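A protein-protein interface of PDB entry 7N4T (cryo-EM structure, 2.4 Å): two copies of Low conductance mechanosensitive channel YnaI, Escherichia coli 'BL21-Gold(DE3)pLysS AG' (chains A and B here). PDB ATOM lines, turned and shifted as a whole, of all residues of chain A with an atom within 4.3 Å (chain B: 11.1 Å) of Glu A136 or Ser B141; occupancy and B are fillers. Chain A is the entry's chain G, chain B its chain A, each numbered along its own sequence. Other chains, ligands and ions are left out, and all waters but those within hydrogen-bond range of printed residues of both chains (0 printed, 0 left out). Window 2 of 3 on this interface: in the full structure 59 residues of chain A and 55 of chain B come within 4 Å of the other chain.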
ATOM      1  N   LEU A 132      11.987  -0.840  22.391  1.00  0.00           N
ATOM      2  CA  LEU A 132      10.607  -0.850  21.922  1.00  0.00           C
ATOM      3  C   LEU A 132       9.741   0.211  22.588  1.00  0.00           C
ATOM      4  O   LEU A 132       8.766   0.668  21.983  1.00  0.00           O
ATOM      5  CB  LEU A 132       9.986  -2.231  22.156  1.00  0.00           C
ATOM      6  CG  LEU A 132       8.533  -2.407  21.704  1.00  0.00           C
ATOM      7  CD1 LEU A 132       8.401  -2.167  20.209  1.00  0.00           C
ATOM      8  CD2 LEU A 132       8.027  -3.792  22.071  1.00  0.00           C
ATOM      9  N   LEU A 133      10.074   0.616  23.814  1.00  0.00           N
ATOM     10  CA  LEU A 133       9.233   1.510  24.600  1.00  0.00           C
ATOM     11  C   LEU A 133       9.741   2.945  24.628  1.00  0.00           C
ATOM     12  O   LEU A 133       8.935   3.878  24.642  1.00  0.00           O
ATOM     13  CB  LEU A 133       9.117   0.990  26.037  1.00  0.00           C
ATOM     14  CG  LEU A 133       8.021   1.629  26.894  1.00  0.00           C
ATOM     15  CD1 LEU A 133       6.640   1.192  26.423  1.00  0.00           C
ATOM     16  CD2 LEU A 133       8.222   1.286  28.361  1.00  0.00           C
ATOM     17  N   TYR A 134      11.056   3.148  24.662  1.00  0.00           N
ATOM     18  CA  TYR A 134      11.634   4.483  24.637  1.00  0.00           C
ATOM     19  C   TYR A 134      12.261   4.829  23.292  1.00  0.00           C
ATOM     20  O   TYR A 134      12.853   5.904  23.159  1.00  0.00           O
ATOM     21  CB  TYR A 134      12.677   4.625  25.750  1.00  0.00           C
ATOM     22  CG  TYR A 134      12.082   5.046  27.074  1.00  0.00           C
ATOM     23  CD1 TYR A 134      11.152   4.245  27.724  1.00  0.00           C
ATOM     24  CD2 TYR A 134      12.443   6.247  27.671  1.00  0.00           C
ATOM     25  CE1 TYR A 134      10.602   4.626  28.934  1.00  0.00           C
ATOM     26  CE2 TYR A 134      11.898   6.635  28.880  1.00  0.00           C
ATOM     27  CZ  TYR A 134      10.979   5.821  29.507  1.00  0.00           C
ATOM     28  OH  TYR A 134      10.434   6.204  30.711  1.00  0.00           O
ATOM     29  N   GLY A 135      12.145   3.951  22.301  1.00  0.00           N
ATOM     30  CA  GLY A 135      12.631   4.217  20.966  1.00  0.00           C
ATOM     31  C   GLY A 135      11.624   4.849  20.035  1.00  0.00           C
ATOM     32  O   GLY A 135      11.926   5.046  18.855  1.00  0.00           O
ATOM     33  N   GLU A 136      10.425   5.174  20.525  1.00  0.00           N
ATOM     34  CA  GLU A 136       9.406   5.751  19.654  1.00  0.00           C
ATOM     35  C   GLU A 136       9.845   7.104  19.111  1.00  0.00           C
ATOM     36  O   GLU A 136       9.639   7.403  17.928  1.00  0.00           O
ATOM     37  CB  GLU A 136       8.083   5.878  20.412  1.00  0.00           C
ATOM     38  CG  GLU A 136       8.125   6.840  21.595  1.00  0.00           C
ATOM     39  CD  GLU A 136       7.713   8.256  21.231  1.00  0.00           C
ATOM     40  OE1 GLU A 136       7.061   8.445  20.182  1.00  0.00           O
ATOM     41  OE2 GLU A 136       8.040   9.184  22.000  1.00  0.00           O
ATOM     42  N   HIS A 137      10.454   7.936  19.955  1.00  0.00           N
ATOM     43  CA  HIS A 137      10.881   9.267  19.534  1.00  0.00           C
ATOM     44  C   HIS A 137      12.286   9.247  18.941  1.00  0.00           C
ATOM     45  O   HIS A 137      12.492   9.714  17.816  1.00  0.00           O
ATOM     46  CB  HIS A 137      10.806  10.251  20.709  1.00  0.00           C
ATOM     47  CG  HIS A 137      11.422   9.742  21.975  1.00  0.00           C
ATOM     48  ND1 HIS A 137      10.761   8.891  22.835  1.00  0.00           N
ATOM     49  CD2 HIS A 137      12.633   9.973  22.534  1.00  0.00           C
ATOM     50  CE1 HIS A 137      11.540   8.615  23.864  1.00  0.00           C
ATOM     51  NE2 HIS A 137      12.683   9.258  23.706  1.00  0.00           N
ATOM     52  N   PHE A 138      13.263   8.715  19.678  1.00  0.00           N
ATOM     53  CA  PHE A 138      14.612   8.606  19.132  1.00  0.00           C
ATOM     54  C   PHE A 138      14.637   7.686  17.919  1.00  0.00           C
ATOM     55  O   PHE A 138      15.290   7.990  16.913  1.00  0.00           O
ATOM     56  CB  PHE A 138      15.579   8.106  20.206  1.00  0.00           C
ATOM     57  CG  PHE A 138      16.127   9.197  21.084  1.00  0.00           C
ATOM     58  CD1 PHE A 138      16.981  10.156  20.567  1.00  0.00           C
ATOM     59  CD2 PHE A 138      15.790   9.259  22.425  1.00  0.00           C
ATOM     60  CE1 PHE A 138      17.487  11.160  21.370  1.00  0.00           C
ATOM     61  CE2 PHE A 138      16.293  10.262  23.234  1.00  0.00           C
ATOM     62  CZ  PHE A 138      17.143  11.213  22.705  1.00  0.00           C
ATOM     63  N   GLY A 139      13.931   6.561  17.993  1.00  0.00           N
ATOM     64  CA  GLY A 139      13.842   5.646  16.873  1.00  0.00           C
ATOM     65  C   GLY A 139      12.657   5.948  15.981  1.00  0.00           C
ATOM     66  O   GLY A 139      11.504   5.753  16.377  1.00  0.00           O
ATOM     67  N   LEU A 142       7.760   4.591  13.466  1.00  0.00           N
ATOM     68  CA  LEU A 142       6.902   3.960  14.464  1.00  0.00           C
ATOM     69  C   LEU A 142       6.265   2.692  13.913  1.00  0.00           C
ATOM     70  O   LEU A 142       6.197   1.670  14.602  1.00  0.00           O
ATOM     71  CB  LEU A 142       5.825   4.941  14.927  1.00  0.00           C
ATOM     72  CG  LEU A 142       6.292   6.057  15.865  1.00  0.00           C
ATOM     73  CD1 LEU A 142       5.207   7.109  16.027  1.00  0.00           C
ATOM     74  CD2 LEU A 142       6.691   5.489  17.218  1.00  0.00           C
ATOM     75  N   VAL B 131      -0.803  -0.521  34.143  1.00  0.00           N
ATOM     76  CA  VAL B 131       0.243   0.004  33.270  1.00  0.00           C
ATOM     77  C   VAL B 131      -0.251   0.081  31.831  1.00  0.00           C
ATOM     78  O   VAL B 131       0.102   1.008  31.091  1.00  0.00           O
ATOM     79  CB  VAL B 131       1.529  -0.837  33.392  1.00  0.00           C
ATOM     80  CG1 VAL B 131       1.367  -2.187  32.721  1.00  0.00           C
ATOM     81  CG2 VAL B 131       2.711  -0.083  32.802  1.00  0.00           C
ATOM     82  N   LEU B 132      -1.073  -0.882  31.404  1.00  0.00           N
ATOM     83  CA  LEU B 132      -1.608  -0.831  30.048  1.00  0.00           C
ATOM     84  C   LEU B 132      -2.633   0.287  29.897  1.00  0.00           C
ATOM     85  O   LEU B 132      -2.643   0.995  28.884  1.00  0.00           O
ATOM     86  CB  LEU B 132      -2.228  -2.177  29.677  1.00  0.00           C
ATOM     87  CG  LEU B 132      -2.808  -2.283  28.264  1.00  0.00           C
ATOM     88  CD1 LEU B 132      -1.750  -1.976  27.216  1.00  0.00           C
ATOM     89  CD2 LEU B 132      -3.405  -3.663  28.035  1.00  0.00           C
ATOM     90  N   TYR B 134      -3.128   3.081  31.885  1.00  0.00           N
ATOM     91  CA  TYR B 134      -2.578   4.401  32.156  1.00  0.00           C
ATOM     92  C   TYR B 134      -1.188   4.588  31.565  1.00  0.00           C
ATOM     93  O   TYR B 134      -0.514   5.570  31.889  1.00  0.00           O
ATOM     94  CB  TYR B 134      -2.542   4.654  33.667  1.00  0.00           C
ATOM     95  CG  TYR B 134      -3.906   4.815  34.312  1.00  0.00           C
ATOM     96  CD1 TYR B 134      -5.076   4.700  33.568  1.00  0.00           C
ATOM     97  CD2 TYR B 134      -4.021   5.087  35.669  1.00  0.00           C
ATOM     98  CE1 TYR B 134      -6.316   4.849  34.157  1.00  0.00           C
ATOM     99  CE2 TYR B 134      -5.259   5.236  36.267  1.00  0.00           C
ATOM    100  CZ  TYR B 134      -6.402   5.117  35.506  1.00  0.00           C
ATOM    101  OH  TYR B 134      -7.636   5.265  36.095  1.00  0.00           O
ATOM    102  N   GLY B 135      -0.744   3.669  30.705  1.00  0.00           N
ATOM    103  CA  GLY B 135       0.576   3.808  30.113  1.00  0.00           C
ATOM    104  C   GLY B 135       0.696   5.030  29.223  1.00  0.00           C
ATOM    105  O   GLY B 135       1.694   5.752  29.277  1.00  0.00           O
ATOM    106  N   GLU B 136      -0.323   5.286  28.399  1.00  0.00           N
ATOM    107  CA  GLU B 136      -0.247   6.400  27.458  1.00  0.00           C
ATOM    108  C   GLU B 136      -0.052   7.727  28.180  1.00  0.00           C
ATOM    109  O   GLU B 136       0.625   8.627  27.670  1.00  0.00           O
ATOM    110  CB  GLU B 136      -1.507   6.446  26.593  1.00  0.00           C
ATOM    111  CG  GLU B 136      -1.470   7.519  25.514  1.00  0.00           C
ATOM    112  CD  GLU B 136      -2.687   7.488  24.612  1.00  0.00           C
ATOM    113  OE1 GLU B 136      -3.597   6.673  24.867  1.00  0.00           O
ATOM    114  OE2 GLU B 136      -2.735   8.281  23.648  1.00  0.00           O
ATOM    115  N   HIS B 137      -0.636   7.869  29.372  1.00  0.00           N
ATOM    116  CA  HIS B 137      -0.515   9.125  30.104  1.00  0.00           C
ATOM    117  C   HIS B 137       0.939   9.428  30.442  1.00  0.00           C
ATOM    118  O   HIS B 137       1.391  10.571  30.306  1.00  0.00           O
ATOM    119  CB  HIS B 137      -1.358   9.073  31.376  1.00  0.00           C
ATOM    120  CG  HIS B 137      -2.819   9.300  31.141  1.00  0.00           C
ATOM    121  ND1 HIS B 137      -3.708   9.546  32.165  1.00  0.00           N
ATOM    122  CD2 HIS B 137      -3.544   9.320  29.999  1.00  0.00           C
ATOM    123  CE1 HIS B 137      -4.920   9.707  31.664  1.00  0.00           C
ATOM    124  NE2 HIS B 137      -4.847   9.575  30.351  1.00  0.00           N
ATOM    125  N   PHE B 138       1.686   8.419  30.884  1.00  0.00           N
ATOM    126  CA  PHE B 138       3.075   8.591  31.290  1.00  0.00           C
ATOM    127  C   PHE B 138       4.034   7.772  30.442  1.00  0.00           C
ATOM    128  O   PHE B 138       5.085   8.281  30.038  1.00  0.00           O
ATOM    129  CB  PHE B 138       3.230   8.222  32.773  1.00  0.00           C
ATOM    130  CG  PHE B 138       2.343   9.019  33.687  1.00  0.00           C
ATOM    131  CD1 PHE B 138       2.782  10.213  34.234  1.00  0.00           C
ATOM    132  CD2 PHE B 138       1.067   8.579  33.991  1.00  0.00           C
ATOM    133  CE1 PHE B 138       1.967  10.950  35.071  1.00  0.00           C
ATOM    134  CE2 PHE B 138       0.246   9.311  34.828  1.00  0.00           C
ATOM    135  CZ  PHE B 138       0.697  10.498  35.369  1.00  0.00           C
ATOM    136  N   GLY B 139       3.705   6.513  30.164  1.00  0.00           N
ATOM    137  CA  GLY B 139       4.542   5.686  29.318  1.00  0.00           C
ATOM    138  C   GLY B 139       4.402   6.035  27.851  1.00  0.00           C
ATOM    139  O   GLY B 139       3.326   5.872  27.266  1.00  0.00           O
ATOM    140  N   MET B 140       5.482   6.514  27.244  1.00  0.00           N
ATOM    141  CA  MET B 140       5.460   6.912  25.844  1.00  0.00           C
ATOM    142  C   MET B 140       5.404   5.660  24.966  1.00  0.00           C
ATOM    143  O   MET B 140       5.276   4.530  25.447  1.00  0.00           O
ATOM    144  CB  MET B 140       6.673   7.780  25.526  1.00  0.00           C
ATOM    145  CG  MET B 140       6.559   9.210  26.026  1.00  0.00           C
ATOM    146  SD  MET B 140       6.742   9.343  27.814  1.00  0.00           S
ATOM    147  CE  MET B 140       8.505   9.085  27.995  1.00  0.00           C
ATOM    148  N   SER B 141       5.501   5.858  23.652  1.00  0.00           N
ATOM    149  CA  SER B 141       5.481   4.764  22.683  1.00  0.00           C
ATOM    150  C   SER B 141       4.156   4.003  22.745  1.00  0.00           C
ATOM    151  O   SER B 141       4.098   2.822  23.094  1.00  0.00           O
ATOM    152  CB  SER B 141       6.665   3.816  22.899  1.00  0.00           C
ATOM    153  OG  SER B 141       6.560   3.135  24.137  1.00  0.00           O
ATOM    154  N   LEU B 142       3.081   4.716  22.406  1.00  0.00           N
ATOM    155  CA  LEU B 142       1.782   4.066  22.280  1.00  0.00           C
ATOM    156  C   LEU B 142       1.880   2.843  21.380  1.00  0.00           C
ATOM    157  O   LEU B 142       1.289   1.797  21.670  1.00  0.00           O
ATOM    158  CB  LEU B 142       0.755   5.061  21.734  1.00  0.00           C
ATOM    159  CG  LEU B 142      -0.708   4.610  21.699  1.00  0.00           C
ATOM    160  CD1 LEU B 142      -1.646   5.806  21.779  1.00  0.00           C
ATOM    161  CD2 LEU B 142      -0.997   3.798  20.444  1.00  0.00           C
ATOM    162  N   SER B 143       2.637   2.951  20.287  1.00  0.00           N
ATOM    163  CA  SER B 143       2.848   1.804  19.410  1.00  0.00           C
ATOM    164  C   SER B 143       3.687   0.729  20.095  1.00  0.00           C
ATOM    165  O   SER B 143       3.381  -0.467  19.994  1.00  0.00           O
ATOM    166  CB  SER B 143       3.515   2.268  18.116  1.00  0.00           C
ATOM    167  OG  SER B 143       3.691   1.195  17.215  1.00  0.00           O
ATOM    168  N   GLY B 144       4.750   1.132  20.792  1.00  0.00           N
ATOM    169  CA  GLY B 144       5.555   0.162  21.515  1.00  0.00           C
ATOM    170  C   GLY B 144       4.782  -0.508  22.634  1.00  0.00           C
ATOM    171  O   GLY B 144       4.911  -1.715  22.859  1.00  0.00           O
ATOM    172  N   LEU B 145       3.972   0.268  23.358  1.00  0.00           N
ATOM    173  CA  LEU B 145       3.112  -0.315  24.379  1.00  0.00           C
ATOM    174  C   LEU B 145       2.116  -1.284  23.757  1.00  0.00           C
ATOM    175  O   LEU B 145       1.845  -2.351  24.317  1.00  0.00           O
ATOM    176  CB  LEU B 145       2.383   0.790  25.143  1.00  0.00           C
ATOM    177  CG  LEU B 145       1.906   0.430  26.550  1.00  0.00           C
ATOM    178  CD1 LEU B 145       3.086   0.257  27.494  1.00  0.00           C
ATOM    179  CD2 LEU B 145       0.948   1.489  27.073  1.00  0.00           C
ATOM    180  N   LEU B 146       1.554  -0.922  22.602  1.00  0.00           N
ATOM    181  CA  LEU B 146       0.677  -1.840  21.884  1.00  0.00           C
ATOM    182  C   LEU B 146       1.386  -3.156  21.608  1.00  0.00           C
ATOM    183  O   LEU B 146       0.852  -4.234  21.888  1.00  0.00           O
ATOM    184  CB  LEU B 146       0.218  -1.207  20.571  1.00  0.00           C
ATOM    185  CG  LEU B 146      -1.019  -0.315  20.632  1.00  0.00           C
ATOM    186  CD1 LEU B 146      -1.204   0.422  19.314  1.00  0.00           C
ATOM    187  CD2 LEU B 146      -2.255  -1.133  20.972  1.00  0.00           C
ATOM    188  N   THR B 147       2.594  -3.086  21.049  1.00  0.00           N
ATOM    189  CA  THR B 147       3.326  -4.304  20.714  1.00  0.00           C
ATOM    190  C   THR B 147       3.583  -5.145  21.958  1.00  0.00           C
ATOM    191  O   THR B 147       3.325  -6.356  21.970  1.00  0.00           O
ATOM    192  CB  THR B 147       4.647  -3.953  20.028  1.00  0.00           C
ATOM    193  OG1 THR B 147       4.384  -3.334  18.764  1.00  0.00           O
ATOM    194  CG2 THR B 147       5.491  -5.201  19.814  1.00  0.00           C
ATOM    195  N   PHE B 148       4.089  -4.516  23.020  1.00  0.00           N
ATOM    196  CA  PHE B 148       4.423  -5.258  24.231  1.00  0.00           C
ATOM    197  C   PHE B 148       3.187  -5.923  24.825  1.00  0.00           C
ATOM    198  O   PHE B 148       3.197  -7.123  25.131  1.00  0.00           O
ATOM    199  CB  PHE B 148       5.076  -4.320  25.247  1.00  0.00           C
ATOM    200  CG  PHE B 148       4.910  -4.757  26.673  1.00  0.00           C
ATOM    201  CD1 PHE B 148       5.735  -5.727  27.215  1.00  0.00           C
ATOM    202  CD2 PHE B 148       3.931  -4.193  27.473  1.00  0.00           C
ATOM    203  CE1 PHE B 148       5.585  -6.129  28.529  1.00  0.00           C
ATOM    204  CE2 PHE B 148       3.776  -4.590  28.787  1.00  0.00           C
ATOM    205  CZ  PHE B 148       4.604  -5.560  29.315  1.00  0.00           C
ATOM    206  N   GLY B 149       2.110  -5.155  24.996  1.00  0.00           N
ATOM    207  CA  GLY B 149       0.902  -5.714  25.576  1.00  0.00           C
ATOM    208  C   GLY B 149       0.302  -6.811  24.723  1.00  0.00           C
ATOM    209  O   GLY B 149      -0.142  -7.837  25.241  1.00  0.00           O
ATOM    210  N   GLY B 150       0.279  -6.614  23.403  1.00  0.00           N
ATOM    211  CA  GLY B 150      -0.256  -7.639  22.528  1.00  0.00           C
ATOM    212  C   GLY B 150       0.536  -8.927  22.596  1.00  0.00           C
ATOM    213  O   GLY B 150      -0.037 -10.014  22.681  1.00  0.00           O
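O of Leu A133 sits at hydrogen-bond distance from OG of Ser B141 (2.5 Å).
The backbone carbonyl oxygen (O) of Ser B143 sits at hydrogen-bond distance from the side-chain hydroxyl (OG1) of Thr B147.
The side-chain carboxylate of Glu A136 sits at hydrogen-bond distance from a ring nitrogen (ND1) of His A137, 2.9 Å away.
Among the printed residues, pairs that only touch across the chains: Leu A132 with Gly B144 (3.3 Å), Glu A136 with Ser B141 (3.5 Å), Leu A142 with Ser B143 (3.7 Å), Leu A132 with Thr B147 (3.7 Å), Leu A133 with Met B140 (3.7 Å), Leu A133 with Leu B145 (3.8 Å) and Leu A132 with Ser B141 (3.9 Å).
Glu A136 touches just one residue of chain B: Ser B141.
Ser B141 touches just these residues of chain A: Leu A132 (3.9 Å), Leu A133 (2.5 Å) and Glu A136 (3.5 Å).
Leu A133 touches three residues of chain B.
No residue of chain B comes within 4 Å of Gly A135.
No residue of chain B comes within 4 Å of His A137.
No residue of chain B comes within 4 Å of Gly A139.
Of the printed residues of chain A, Met B140 touches Leu A133.
Of the printed residues of chain A, Ser B143 touches Leu A142 (3.7 Å).
Tyr B134 touches none of the printed residues of chain A.
The nearest printed residue of chain A that does not touch Ser B141 is Tyr A134 (4.5 Å).
Of the 19 printed residues of chain B, 6 touch a printed residue of chain A.
Printed residues of chain B that touch a printed residue of chain A: Met B140, Ser B141, Ser B143, Gly B144, Leu B145 and Thr B147.
Hydrophobic or aromatic side chains of chain B within 4 Å of the printed part of chain A: Leu B145.
Of the 9 printed residues of chain A, 4 touch a printed residue of chain B.
Printed residues of chain A that touch a printed residue of chain B: Leu A132, Leu A133, Glu A136 and Leu A142.
Along chain A the printed residues that touch a printed residue of chain B span positions 132 to 142.
Among the printed residues, 8 pairs touch across the chains.
Among the printed residues, no Asp or Glu carboxylate lies within 4 Å of a Lys or Arg side-chain nitrogen of the other chain.
Positions printed for both chains: 132, 134, 135, 136, 137, 138, 139 and 142.
Of the 8 pairs that touch across the chains among the printed residues, none has its exchanged pair printed and touching as well.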
